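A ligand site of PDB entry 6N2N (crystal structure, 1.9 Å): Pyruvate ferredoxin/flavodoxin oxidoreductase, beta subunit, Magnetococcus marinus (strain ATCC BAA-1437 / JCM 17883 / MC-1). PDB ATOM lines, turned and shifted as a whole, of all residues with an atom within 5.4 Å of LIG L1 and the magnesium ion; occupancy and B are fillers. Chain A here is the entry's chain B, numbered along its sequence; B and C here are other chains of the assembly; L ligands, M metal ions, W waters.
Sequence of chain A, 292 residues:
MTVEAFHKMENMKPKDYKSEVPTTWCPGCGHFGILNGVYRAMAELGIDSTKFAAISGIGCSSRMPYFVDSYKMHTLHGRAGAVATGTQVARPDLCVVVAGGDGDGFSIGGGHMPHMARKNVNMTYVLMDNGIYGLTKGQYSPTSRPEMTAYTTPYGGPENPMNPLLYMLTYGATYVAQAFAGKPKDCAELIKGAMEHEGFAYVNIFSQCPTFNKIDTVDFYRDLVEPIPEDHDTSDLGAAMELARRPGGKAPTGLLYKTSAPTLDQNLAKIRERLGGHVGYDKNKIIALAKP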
ATOM      1  N   HIS A  31     -29.266 -14.366 -17.638  1.00  0.00           N
ATOM      2  CA  HIS A  31     -30.004 -13.901 -16.467  1.00  0.00           C
ATOM      3  C   HIS A  31     -31.140 -14.849 -16.081  1.00  0.00           C
ATOM      4  O   HIS A  31     -31.533 -14.875 -14.914  1.00  0.00           O
ATOM      5  CB  HIS A  31     -30.552 -12.490 -16.704  1.00  0.00           C
ATOM      6  CG  HIS A  31     -29.500 -11.445 -16.906  1.00  0.00           C
ATOM      7  ND1 HIS A  31     -28.177 -11.638 -16.581  1.00  0.00           N
ATOM      8  CD2 HIS A  31     -29.578 -10.188 -17.428  1.00  0.00           C
ATOM      9  CE1 HIS A  31     -27.484 -10.543 -16.881  1.00  0.00           C
ATOM     10  NE2 HIS A  31     -28.314  -9.650 -17.390  1.00  0.00           N
ATOM     11  N   ILE A  58     -30.136   0.036 -12.530  1.00  0.00           N
ATOM     12  CA  ILE A  58     -30.564   0.022 -13.932  1.00  0.00           C
ATOM     13  C   ILE A  58     -29.648  -0.910 -14.720  1.00  0.00           C
ATOM     14  O   ILE A  58     -28.438  -0.951 -14.493  1.00  0.00           O
ATOM     15  CB  ILE A  58     -30.559   1.428 -14.566  1.00  0.00           C
ATOM     16  CG1 ILE A  58     -31.297   2.442 -13.683  1.00  0.00           C
ATOM     17  CG2 ILE A  58     -31.236   1.390 -15.936  1.00  0.00           C
ATOM     18  CD1 ILE A  58     -32.785   2.238 -13.642  1.00  0.00           C
ATOM     19  N   GLY A  59     -30.241  -1.659 -15.627  1.00  0.00           N
ATOM     20  CA  GLY A  59     -29.562  -2.655 -16.431  1.00  0.00           C
ATOM     21  C   GLY A  59     -30.514  -3.807 -16.697  1.00  0.00           C
ATOM     22  O   GLY A  59     -31.564  -3.933 -16.066  1.00  0.00           O
ATOM     23  N   CYS A  60     -30.151  -4.647 -17.665  1.00  0.00           N
ATOM     24  CA  CYS A  60     -30.928  -5.869 -17.892  1.00  0.00           C
ATOM     25  C   CYS A  60     -30.969  -6.712 -16.628  1.00  0.00           C
ATOM     26  O   CYS A  60     -32.030  -7.182 -16.205  1.00  0.00           O
ATOM     27  CB  CYS A  60     -30.330  -6.685 -19.044  1.00  0.00           C
ATOM     28  SG  CYS A  60     -30.540  -5.954 -20.690  1.00  0.00           S
ATOM     29  N   SER A  61     -29.805  -6.909 -15.994  1.00  0.00           N
ATOM     30  CA  SER A  61     -29.745  -7.624 -14.732  1.00  0.00           C
ATOM     31  C   SER A  61     -30.722  -7.042 -13.716  1.00  0.00           C
ATOM     32  O   SER A  61     -31.468  -7.773 -13.061  1.00  0.00           O
ATOM     33  CB  SER A  61     -28.321  -7.570 -14.177  1.00  0.00           C
ATOM     34  OG  SER A  61     -28.265  -8.136 -12.887  1.00  0.00           O
ATOM     35  N   SER A  62     -30.769  -5.703 -13.623  1.00  0.00           N
ATOM     36  CA  SER A  62     -31.526  -4.987 -12.613  1.00  0.00           C
ATOM     37  C   SER A  62     -33.035  -5.137 -12.760  1.00  0.00           C
ATOM     38  O   SER A  62     -33.771  -4.699 -11.873  1.00  0.00           O
ATOM     39  CB  SER A  62     -31.152  -3.501 -12.669  1.00  0.00           C
ATOM     40  OG  SER A  62     -29.761  -3.317 -12.467  1.00  0.00           O
ATOM     41  N   HIS A  77     -29.320   4.083 -11.294  1.00  0.00           N
ATOM     42  CA  HIS A  77     -28.172   3.336 -11.789  1.00  0.00           C
ATOM     43  C   HIS A  77     -26.986   3.480 -10.830  1.00  0.00           C
ATOM     44  O   HIS A  77     -26.506   4.590 -10.580  1.00  0.00           O
ATOM     45  CB  HIS A  77     -27.818   3.852 -13.179  1.00  0.00           C
ATOM     46  CG  HIS A  77     -26.759   3.068 -13.903  1.00  0.00           C
ATOM     47  ND1 HIS A  77     -26.647   1.691 -13.807  1.00  0.00           N
ATOM     48  CD2 HIS A  77     -25.785   3.465 -14.750  1.00  0.00           C
ATOM     49  CE1 HIS A  77     -25.631   1.289 -14.552  1.00  0.00           C
ATOM     50  NE2 HIS A  77     -25.086   2.349 -15.133  1.00  0.00           N
ATOM     51  N   GLY A 100     -27.895  -6.905  -9.719  1.00  0.00           N
ATOM     52  CA  GLY A 100     -27.459  -5.940 -10.707  1.00  0.00           C
ATOM     53  C   GLY A 100     -26.274  -6.481 -11.489  1.00  0.00           C
ATOM     54  O   GLY A 100     -25.678  -7.493 -11.121  1.00  0.00           O
ATOM     55  N   GLY A 101     -25.925  -5.750 -12.550  1.00  0.00           N
ATOM     56  CA  GLY A 101     -24.919  -6.199 -13.476  1.00  0.00           C
ATOM     57  C   GLY A 101     -23.532  -5.651 -13.176  1.00  0.00           C
ATOM     58  O   GLY A 101     -23.294  -4.965 -12.187  1.00  0.00           O
ATOM     59  N   ASP A 102     -22.598  -5.977 -14.074  1.00  0.00           N
ATOM     60  CA  ASP A 102     -21.212  -5.590 -13.844  1.00  0.00           C
ATOM     61  C   ASP A 102     -20.998  -4.085 -13.980  1.00  0.00           C
ATOM     62  O   ASP A 102     -20.180  -3.505 -13.253  1.00  0.00           O
ATOM     63  CB  ASP A 102     -20.286  -6.371 -14.792  1.00  0.00           C
ATOM     64  CG  ASP A 102     -20.865  -6.533 -16.205  1.00  0.00           C
ATOM     65  OD1 ASP A 102     -22.075  -6.794 -16.368  1.00  0.00           O
ATOM     66  OD2 ASP A 102     -20.074  -6.403 -17.160  1.00  0.00           O
ATOM     67  N   GLY A 103     -21.731  -3.421 -14.885  1.00  0.00           N
ATOM     68  CA  GLY A 103     -21.587  -1.986 -15.005  1.00  0.00           C
ATOM     69  C   GLY A 103     -22.270  -1.223 -13.882  1.00  0.00           C
ATOM     70  O   GLY A 103     -21.689  -0.302 -13.280  1.00  0.00           O
ATOM     71  N   ASP A 104     -23.513  -1.604 -13.595  1.00  0.00           N
ATOM     72  CA  ASP A 104     -24.251  -1.021 -12.487  1.00  0.00           C
ATOM     73  C   ASP A 104     -23.484  -1.143 -11.168  1.00  0.00           C
ATOM     74  O   ASP A 104     -23.483  -0.209 -10.356  1.00  0.00           O
ATOM     75  CB  ASP A 104     -25.618  -1.703 -12.394  1.00  0.00           C
ATOM     76  CG  ASP A 104     -26.489  -1.137 -11.292  1.00  0.00           C
ATOM     77  OD1 ASP A 104     -27.100  -0.072 -11.494  1.00  0.00           O
ATOM     78  OD2 ASP A 104     -26.594  -1.784 -10.228  1.00  0.00           O
ATOM     79  N   GLY A 105     -22.833  -2.282 -10.950  1.00  0.00           N
ATOM     80  CA  GLY A 105     -22.164  -2.551  -9.692  1.00  0.00           C
ATOM     81  C   GLY A 105     -20.767  -1.960  -9.564  1.00  0.00           C
ATOM     82  O   GLY A 105     -20.410  -1.417  -8.517  1.00  0.00           O
ATOM     83  N   ILE A 108     -20.507   2.784 -12.335  1.00  0.00           N
ATOM     84  CA  ILE A 108     -21.122   3.877 -11.593  1.00  0.00           C
ATOM     85  C   ILE A 108     -21.361   3.495 -10.129  1.00  0.00           C
ATOM     86  O   ILE A 108     -21.341   4.357  -9.251  1.00  0.00           O
ATOM     87  CB  ILE A 108     -22.429   4.317 -12.273  1.00  0.00           C
ATOM     88  CG1 ILE A 108     -22.997   5.562 -11.598  1.00  0.00           C
ATOM     89  CG2 ILE A 108     -23.442   3.165 -12.286  1.00  0.00           C
ATOM     90  CD1 ILE A 108     -24.069   6.260 -12.396  1.00  0.00           C
ATOM     91  N   MET A 128     -24.587 -10.095 -11.657  1.00  0.00           N
ATOM     92  CA  MET A 128     -24.769 -10.886 -12.866  1.00  0.00           C
ATOM     93  C   MET A 128     -23.796 -10.370 -13.924  1.00  0.00           C
ATOM     94  O   MET A 128     -24.071  -9.390 -14.609  1.00  0.00           O
ATOM     95  CB  MET A 128     -26.219 -10.807 -13.317  1.00  0.00           C
ATOM     96  CG  MET A 128     -27.186 -11.003 -12.164  1.00  0.00           C
ATOM     97  SD  MET A 128     -28.896 -11.174 -12.683  1.00  0.00           S
ATOM     98  CE  MET A 128     -29.708 -10.614 -11.212  1.00  0.00           C
ATOM     99  N   ASN A 130     -21.951 -10.238 -17.179  1.00  0.00           N
ATOM    100  CA  ASN A 130     -21.981 -10.620 -18.583  1.00  0.00           C
ATOM    101  C   ASN A 130     -20.879  -9.945 -19.405  1.00  0.00           C
ATOM    102  O   ASN A 130     -20.856 -10.095 -20.623  1.00  0.00           O
ATOM    103  CB  ASN A 130     -23.359 -10.352 -19.224  1.00  0.00           C
ATOM    104  CG  ASN A 130     -23.822  -8.923 -19.072  1.00  0.00           C
ATOM    105  OD1 ASN A 130     -23.045  -8.037 -18.717  1.00  0.00           O
ATOM    106  ND2 ASN A 130     -25.109  -8.699 -19.360  1.00  0.00           N
ATOM    107  N   GLY A 131     -19.970  -9.226 -18.747  1.00  0.00           N
ATOM    108  CA  GLY A 131     -18.841  -8.635 -19.437  1.00  0.00           C
ATOM    109  C   GLY A 131     -19.196  -7.535 -20.415  1.00  0.00           C
ATOM    110  O   GLY A 131     -18.437  -7.298 -21.357  1.00  0.00           O
ATOM    111  N   ILE A 132     -20.322  -6.863 -20.218  1.00  0.00           N
ATOM    112  CA  ILE A 132     -20.799  -5.859 -21.164  1.00  0.00           C
ATOM    113  C   ILE A 132     -21.924  -5.047 -20.531  1.00  0.00           C
ATOM    114  O   ILE A 132     -22.480  -5.444 -19.498  1.00  0.00           O
ATOM    115  CB  ILE A 132     -21.243  -6.532 -22.478  1.00  0.00           C
ATOM    116  CG1 ILE A 132     -21.157  -5.554 -23.657  1.00  0.00           C
ATOM    117  CG2 ILE A 132     -22.639  -7.134 -22.338  1.00  0.00           C
ATOM    118  CD1 ILE A 132     -21.108  -6.230 -25.012  1.00  0.00           C
ATOM    119  N   TYR A 133     -22.262  -3.898 -21.129  1.00  0.00           N
ATOM    120  CA  TYR A 133     -23.494  -3.176 -20.787  1.00  0.00           C
ATOM    121  C   TYR A 133     -24.580  -3.644 -21.749  1.00  0.00           C
ATOM    122  O   TYR A 133     -24.623  -3.219 -22.901  1.00  0.00           O
ATOM    123  CB  TYR A 133     -23.309  -1.673 -20.899  1.00  0.00           C
ATOM    124  CG  TYR A 133     -22.263  -1.040 -20.005  1.00  0.00           C
ATOM    125  CD1 TYR A 133     -21.678  -1.750 -18.965  1.00  0.00           C
ATOM    126  CD2 TYR A 133     -21.871   0.281 -20.195  1.00  0.00           C
ATOM    127  CE1 TYR A 133     -20.715  -1.150 -18.146  1.00  0.00           C
ATOM    128  CE2 TYR A 133     -20.919   0.886 -19.389  1.00  0.00           C
ATOM    129  CZ  TYR A 133     -20.344   0.155 -18.373  1.00  0.00           C
ATOM    130  OH  TYR A 133     -19.405   0.761 -17.571  1.00  0.00           O
ATOM    131  N   GLY A 134     -25.474  -4.492 -21.250  1.00  0.00           N
ATOM    132  CA  GLY A 134     -26.536  -5.015 -22.114  1.00  0.00           C
ATOM    133  C   GLY A 134     -27.614  -3.995 -22.400  1.00  0.00           C
ATOM    134  O   GLY A 134     -27.949  -3.744 -23.566  1.00  0.00           O
ATOM    135  N   LEU A 135     -28.168  -3.379 -21.354  1.00  0.00           N
ATOM    136  CA  LEU A 135     -29.395  -2.602 -21.509  1.00  0.00           C
ATOM    137  C   LEU A 135     -29.180  -1.385 -22.406  1.00  0.00           C
ATOM    138  O   LEU A 135     -30.085  -1.005 -23.160  1.00  0.00           O
ATOM    139  CB  LEU A 135     -29.953  -2.175 -20.158  1.00  0.00           C
ATOM    140  CG  LEU A 135     -31.304  -1.461 -20.211  1.00  0.00           C
ATOM    141  CD1 LEU A 135     -32.375  -2.354 -20.850  1.00  0.00           C
ATOM    142  CD2 LEU A 135     -31.743  -1.003 -18.829  1.00  0.00           C
ATOM    143  N   THR A 136     -28.004  -0.765 -22.350  1.00  0.00           N
ATOM    144  CA  THR A 136     -27.680   0.372 -23.211  1.00  0.00           C
ATOM    145  C   THR A 136     -27.173  -0.046 -24.588  1.00  0.00           C
ATOM    146  O   THR A 136     -26.693   0.812 -25.334  1.00  0.00           O
ATOM    147  CB  THR A 136     -26.666   1.290 -22.524  1.00  0.00           C
ATOM    148  OG1 THR A 136     -25.612   0.499 -21.965  1.00  0.00           O
ATOM    149  CG2 THR A 136     -27.353   2.051 -21.414  1.00  0.00           C
ATOM    150  N   SER A 141     -17.541  -3.036 -20.355  1.00  0.00           N
ATOM    151  CA  SER A 141     -17.684  -2.913 -18.916  1.00  0.00           C
ATOM    152  C   SER A 141     -16.341  -3.134 -18.243  1.00  0.00           C
ATOM    153  O   SER A 141     -15.358  -3.507 -18.895  1.00  0.00           O
ATOM    154  CB  SER A 141     -18.706  -3.943 -18.413  1.00  0.00           C
ATOM    155  OG  SER A 141     -18.091  -5.194 -18.153  1.00  0.00           O
ATOM    156  N   TYR B 224     -20.146   8.574 -20.497  1.00  0.00           N
ATOM    157  CA  TYR B 224     -20.677   7.347 -19.937  1.00  0.00           C
ATOM    158  C   TYR B 224     -21.973   7.059 -20.688  1.00  0.00           C
ATOM    159  O   TYR B 224     -22.759   7.984 -20.940  1.00  0.00           O
ATOM    160  CB  TYR B 224     -20.927   7.512 -18.425  1.00  0.00           C
ATOM    161  CG  TYR B 224     -21.270   6.228 -17.691  1.00  0.00           C
ATOM    162  CD1 TYR B 224     -20.346   5.199 -17.585  1.00  0.00           C
ATOM    163  CD2 TYR B 224     -22.509   6.073 -17.101  1.00  0.00           C
ATOM    164  CE1 TYR B 224     -20.660   4.034 -16.915  1.00  0.00           C
ATOM    165  CE2 TYR B 224     -22.827   4.917 -16.417  1.00  0.00           C
ATOM    166  CZ  TYR B 224     -21.904   3.903 -16.328  1.00  0.00           C
ATOM    167  OH  TYR B 224     -22.225   2.758 -15.652  1.00  0.00           O
ATOM    168  N   PRO B 225     -22.195   5.827 -21.120  1.00  0.00           N
ATOM    169  CA  PRO B 225     -23.367   5.544 -21.963  1.00  0.00           C
ATOM    170  C   PRO B 225     -24.661   5.840 -21.210  1.00  0.00           C
ATOM    171  O   PRO B 225     -24.809   5.506 -20.036  1.00  0.00           O
ATOM    172  CB  PRO B 225     -23.232   4.047 -22.276  1.00  0.00           C
ATOM    173  CG  PRO B 225     -21.793   3.742 -22.075  1.00  0.00           C
ATOM    174  CD  PRO B 225     -21.322   4.645 -20.961  1.00  0.00           C
ATOM    175  N   ILE B 226     -25.597   6.465 -21.914  1.00  0.00           N
ATOM    176  CA  ILE B 226     -26.951   6.685 -21.407  1.00  0.00           C
ATOM    177  C   ILE B 226     -27.865   6.970 -22.580  1.00  0.00           C
ATOM    178  O   ILE B 226     -27.521   7.712 -23.501  1.00  0.00           O
ATOM    179  CB  ILE B 226     -26.986   7.826 -20.359  1.00  0.00           C
ATOM    180  CG1 ILE B 226     -28.394   7.924 -19.729  1.00  0.00           C
ATOM    181  CG2 ILE B 226     -26.579   9.162 -20.970  1.00  0.00           C
ATOM    182  CD1 ILE B 226     -28.476   8.956 -18.607  1.00  0.00           C
ATOM    183  N   THR B 227     -29.057   6.368 -22.531  1.00  0.00           N
ATOM    184  CA  THR B 227     -30.076   6.631 -23.532  1.00  0.00           C
ATOM    185  C   THR B 227     -30.695   8.011 -23.294  1.00  0.00           C
ATOM    186  O   THR B 227     -30.944   8.382 -22.148  1.00  0.00           O
ATOM    187  CB  THR B 227     -31.162   5.537 -23.454  1.00  0.00           C
ATOM    188  OG1 THR B 227     -30.555   4.271 -23.670  1.00  0.00           O
ATOM    189  CG2 THR B 227     -32.266   5.735 -24.489  1.00  0.00           C
ATOM    190  N   GLU B 253     -20.766   9.679 -14.982  1.00  0.00           N
ATOM    191  CA  GLU B 253     -20.838  11.027 -15.520  1.00  0.00           C
ATOM    192  C   GLU B 253     -19.981  12.005 -14.734  1.00  0.00           C
ATOM    193  O   GLU B 253     -19.441  12.961 -15.304  1.00  0.00           O
ATOM    194  CB  GLU B 253     -22.285  11.531 -15.536  1.00  0.00           C
ATOM    195  CG  GLU B 253     -23.146  10.901 -16.606  1.00  0.00           C
ATOM    196  CD  GLU B 253     -23.799   9.606 -16.151  1.00  0.00           C
ATOM    197  OE1 GLU B 253     -24.590   9.059 -16.935  1.00  0.00           O
ATOM    198  OE2 GLU B 253     -23.532   9.164 -15.011  1.00  0.00           O
ATOM    199  N   PRO B 277     -30.485  12.601 -16.301  1.00  0.00           N
ATOM    200  CA  PRO B 277     -29.834  12.053 -15.090  1.00  0.00           C
ATOM    201  C   PRO B 277     -28.355  12.364 -15.020  1.00  0.00           C
ATOM    202  O   PRO B 277     -27.841  12.707 -13.938  1.00  0.00           O
ATOM    203  CB  PRO B 277     -30.104  10.545 -15.213  1.00  0.00           C
ATOM    204  CG  PRO B 277     -31.359  10.447 -16.050  1.00  0.00           C
ATOM    205  CD  PRO B 277     -31.268  11.578 -17.025  1.00  0.00           C
ATOM    206  N   GLY B 278     -27.658  12.277 -16.145  1.00  0.00           N
ATOM    207  CA  GLY B 278     -26.234  12.569 -16.147  1.00  0.00           C
ATOM    208  C   GLY B 278     -25.942  14.031 -15.912  1.00  0.00           C
ATOM    209  O   GLY B 278     -24.995  14.371 -15.188  1.00  0.00           O
ATOM    210  N   LEU B 281     -26.051  14.740 -12.251  1.00  0.00           N
ATOM    211  CA  LEU B 281     -24.835  14.334 -11.553  1.00  0.00           C
ATOM    212  C   LEU B 281     -23.677  15.292 -11.813  1.00  0.00           C
ATOM    213  O   LEU B 281     -22.804  15.433 -10.949  1.00  0.00           O
ATOM    214  CB  LEU B 281     -24.446  12.914 -11.953  1.00  0.00           C
ATOM    215  CG  LEU B 281     -25.384  11.811 -11.453  1.00  0.00           C
ATOM    216  CD1 LEU B 281     -25.078  10.508 -12.161  1.00  0.00           C
ATOM    217  CD2 LEU B 281     -25.225  11.662  -9.939  1.00  0.00           C
ATOM    218  N   ARG B 303     -34.490  13.634 -22.477  1.00  0.00           N
ATOM    219  CA  ARG B 303     -35.425  12.521 -22.539  1.00  0.00           C
ATOM    220  C   ARG B 303     -36.558  12.769 -21.547  1.00  0.00           C
ATOM    221  O   ARG B 303     -36.587  13.797 -20.854  1.00  0.00           O
ATOM    222  CB  ARG B 303     -34.719  11.188 -22.238  1.00  0.00           C
ATOM    223  CG  ARG B 303     -34.342  11.004 -20.768  1.00  0.00           C
ATOM    224  CD  ARG B 303     -33.414   9.813 -20.549  1.00  0.00           C
ATOM    225  NE  ARG B 303     -33.618   9.186 -19.247  1.00  0.00           N
ATOM    226  CZ  ARG B 303     -32.987   8.080 -18.851  1.00  0.00           C
ATOM    227  NH1 ARG B 303     -32.088   7.511 -19.648  1.00  0.00           N
ATOM    228  NH2 ARG B 303     -33.244   7.538 -17.667  1.00  0.00           N
ATOM    229  N   GLU C 284     -29.781  14.151  -8.513  1.00  0.00           N
ATOM    230  CA  GLU C 284     -30.379  12.994  -9.176  1.00  0.00           C
ATOM    231  C   GLU C 284     -31.264  12.207  -8.215  1.00  0.00           C
ATOM    232  O   GLU C 284     -32.404  11.862  -8.540  1.00  0.00           O
ATOM    233  CB  GLU C 284     -29.308  12.083  -9.779  1.00  0.00           C
ATOM    234  CG  GLU C 284     -29.880  11.226 -10.940  1.00  0.00           C
ATOM    235  CD  GLU C 284     -29.188   9.873 -11.143  1.00  0.00           C
ATOM    236  OE1 GLU C 284     -28.245   9.546 -10.399  1.00  0.00           O
ATOM    237  OE2 GLU C 284     -29.623   9.141 -12.057  1.00  0.00           O
HETATM  238  N1  LIG L   1     -26.045   6.971 -16.177  1.00  0.00           N
HETATM  239  C1  LIG L   1     -27.016   7.137 -15.303  1.00  0.00           C
HETATM  240  C2  LIG L   1     -26.828   8.167 -14.172  1.00  0.00           C
HETATM  241  N2  LIG L   1     -28.125   6.429 -15.363  1.00  0.00           N
HETATM  242  C3  LIG L   1     -28.319   5.519 -16.342  1.00  0.00           C
HETATM  243  N3  LIG L   1     -29.539   4.784 -16.382  1.00  0.00           N
HETATM  244  C4  LIG L   1     -27.307   5.302 -17.293  1.00  0.00           C
HETATM  245  C5  LIG L   1     -26.141   6.089 -17.180  1.00  0.00           C
HETATM  246  C6  LIG L   1     -27.444   4.272 -18.475  1.00  0.00           C
HETATM  247  N4  LIG L   1     -27.335   2.884 -18.170  1.00  0.00           N
HETATM  248  C7  LIG L   1     -28.394   2.023 -17.892  1.00  0.00           C
HETATM  249  S1  LIG L   1     -28.051   0.449 -17.633  1.00  0.00           S
HETATM  250  C8  LIG L   1     -26.479   0.813 -17.885  1.00  0.00           C
HETATM  251  C9  LIG L   1     -26.188   2.144 -18.184  1.00  0.00           C
HETATM  252  C10 LIG L   1     -24.781   2.672 -18.455  1.00  0.00           C
HETATM  253  C11 LIG L   1     -25.422  -0.280 -17.796  1.00  0.00           C
HETATM  254  C12 LIG L   1     -26.007  -1.715 -17.937  1.00  0.00           C
HETATM  255  O1  LIG L   1     -24.910  -2.634 -17.783  1.00  0.00           O
HETATM  256  P1  LIG L   1     -24.959  -3.699 -16.629  1.00  0.00           P
HETATM  257  O2  LIG L   1     -25.040  -3.056 -15.275  1.00  0.00           O
HETATM  258  O3  LIG L   1     -23.706  -4.537 -16.729  1.00  0.00           O
HETATM  259  O4  LIG L   1     -26.264  -4.595 -16.732  1.00  0.00           O
HETATM  260  P2  LIG L   1     -26.665  -5.513 -17.988  1.00  0.00           P
HETATM  261  O5  LIG L   1     -27.322  -6.727 -17.397  1.00  0.00           O
HETATM  262  O6  LIG L   1     -25.406  -5.842 -18.757  1.00  0.00           O
HETATM  263  O7  LIG L   1     -27.619  -4.747 -18.866  1.00  0.00           O
HETATM  264 FE1  LG2 L   2     -27.937  -9.148 -23.196  1.00  0.00          FE
HETATM  265 FE2  LG2 L   2     -29.748 -10.525 -21.660  1.00  0.00          FE
HETATM  266 FE3  LG2 L   2     -29.943  -7.805 -21.912  1.00  0.00          FE
HETATM  267 FE4  LG2 L   2     -30.551  -9.433 -24.021  1.00  0.00          FE
HETATM  268  S1  LG2 L   2     -31.652  -9.324 -22.030  1.00  0.00           S
HETATM  269  S2  LG2 L   2     -29.280  -7.527 -24.064  1.00  0.00           S
HETATM  270  S3  LG2 L   2     -29.028 -11.098 -23.749  1.00  0.00           S
HETATM  271  S4  LG2 L   2     -28.230  -8.972 -20.941  1.00  0.00           S
HETATM  272 MG    MG M   1     -23.562  -6.285 -17.819  1.00  0.00          MG
HETATM  273  O   HOH W   1     -29.765   6.518 -12.856  1.00  0.00           O
HETATM  274  O   HOH W   2     -24.651  -7.529 -16.553  1.00  0.00           O
HETATM  275  O   HOH W   3     -27.532  -3.926 -13.965  1.00  0.00           O
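The side-chain carboxylate of Asp 104 lies within hydrogen-bond range of the backbone NH of Ile 58.
The backbone NH of Ser 61 is in hydrogen-bond range of a ring nitrogen (NE2) of His 31, 3.4 Å away.
The side-chain hydroxyl (OG) of Ser 61 is in hydrogen-bond range of the side-chain sulfur (SD) of Met 128 (3.1 Å).
The side-chain sulfur (SG) of Cys 60 sits close to the backbone NH (N) of Leu 135 (3.6 Å).
A ring nitrogen (NE2) of His 77 is in hydrogen-bond range of the side-chain hydroxyl (OH) of Tyr 224 of chain B, 2.9 Å away.
The backbone NH (N) of Ile 108 lies within hydrogen-bond range of the backbone carbonyl oxygen (O) of Gly 103 (3.4 Å).
The side-chain hydroxyl (OG) of Ser 141 is in hydrogen-bond range of the backbone NH (N) of Ile 132.
OG of Ser 61 sits close to O of Gly 100, at 3.2 Å.
O of Ile 58 lies close to S1 of LIG L1 (3.5 Å).
His 77 touches LIG L1.
Gly 101 touches LIG L1.
Ile 108 touches LIG L1.
CA of Tyr 133 touches O1 of LIG L1, at 3.4 Å.
Thr 136 touches LIG L1 (CG2 to N4, 3.3 Å).
CE2 of Tyr 224 of chain B touches C5 of LIG L1, 3.6 Å away.
Pro 225 of chain B touches LIG L1 (O to C5, 3.2 Å).
Ile 226 of chain B touches LIG L1 (CB to C5, 3.7 Å).
Leu 281 of chain B touches LIG L1.
Glu 284 of chain C touches LIG L1 (OE2 to C2, 3.6 Å).
Within 4 Å of LIG L1: His 31, Ile 58, Gly 59, Cys 60, Ser 61, His 77, Gly 101, Asp 102, Gly 103, Asp 104, Ile 108, Asn 130, Ile 132, Tyr 133, Gly 134, Leu 135, Thr 136, Tyr 224 of chain B, Pro 225 of chain B, Ile 226 of chain B, Glu 253 of chain B, Leu 281 of chain B and Glu 284 of chain C.
Along chain A the residues within 4 Å of LIG L1 span positions 31 to 136.
The nearest printed residue that does not touch LIG L1 is Pro 277 of chain B (4.2 Å).
Of the 33 residues printed, 3 come within 4 Å of the magnesium ion.
The nearest printed residue that does not touch the magnesium ion is Tyr 133 (4.3 Å).
An iron atom (FE3) of LG2 L2 is bound by the side-chain sulfur (SG) of Cys 60.
O5 of LIG L1 lies within hydrogen-bond range of NE2 of His 31 (3.1 Å).
N of Gly 134 is in hydrogen-bond range of O7 of LIG L1 (3.2 Å).
N of Gly 59 sits close to S1 of LIG L1 (3.6 Å).
An oxygen (O2) of LIG L1 sits at hydrogen-bond distance from the backbone NH of Asp 104 (2.7 Å).
NE2 of His 31 lies close to S4 of LG2 L2 (3.6 Å).
The side-chain carboxylate (OE1) of Glu 253 of chain B sits at hydrogen-bond distance from a nitrogen (N1) of LIG L1 (2.7 Å).
The backbone NH of Leu 135 sits at hydrogen-bond distance from an oxygen (O7) of LIG L1, at 2.9 Å.
O7 of LIG L1 is in hydrogen-bond range of N of Cys 60, 2.8 Å away.
The backbone NH (N) of Gly 103 sits at hydrogen-bond distance from an oxygen (O2) of LIG L1 (3.4 Å).
ND2 of Asn 130 lies close to S4 of LG2 L2, at 3.5 Å.
N of Asp 102 lies close to O3 of LIG L1 (3.2 Å).
The backbone NH of Ser 61 lies within hydrogen-bond range of an oxygen (O5) of LIG L1.
The side-chain sulfur (SG) of Cys 60 lies close to an oxygen (O7) of LIG L1 (3.6 Å).
The magnesium ion is bound by the side-chain amide oxygen (OD1) of Asn 130 (2.0 Å), an oxygen (O3) of LIG L1 (2.1 Å), water W2 (2.1 Å), an oxygen (O6) of LIG L1 (2.1 Å), the side-chain carboxylate (OD1) of Asp 102 (2.1 Å) and the backbone carbonyl oxygen (O) of Ile 132 (2.2 Å).
The magnesium ion has six donor atoms within binding distance.
Water W2 lies within hydrogen-bond range of the backbone carbonyl oxygen of Met 128 (2.8 Å), an oxygen (O5) of LIG L1 (2.9 Å) and the side-chain amide nitrogen of Asn 130 (3.1 Å).
Water W3 lies within hydrogen-bond range of the side-chain hydroxyl (OG) of Ser 62 (2.8 Å), the backbone NH (N) of Gly 101 (2.8 Å), an oxygen (O2) of LIG L1 (2.9 Å) and the backbone carbonyl oxygen (O) of Ile 58 (3.2 Å).
Water W1 lies within hydrogen-bond range of the side-chain carboxylate (OE2) of Glu 284 of chain C (2.7 Å), the backbone NH (N) of His 77 (2.9 Å) and a nitrogen (N2) of LIG L1 (3.0 Å).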
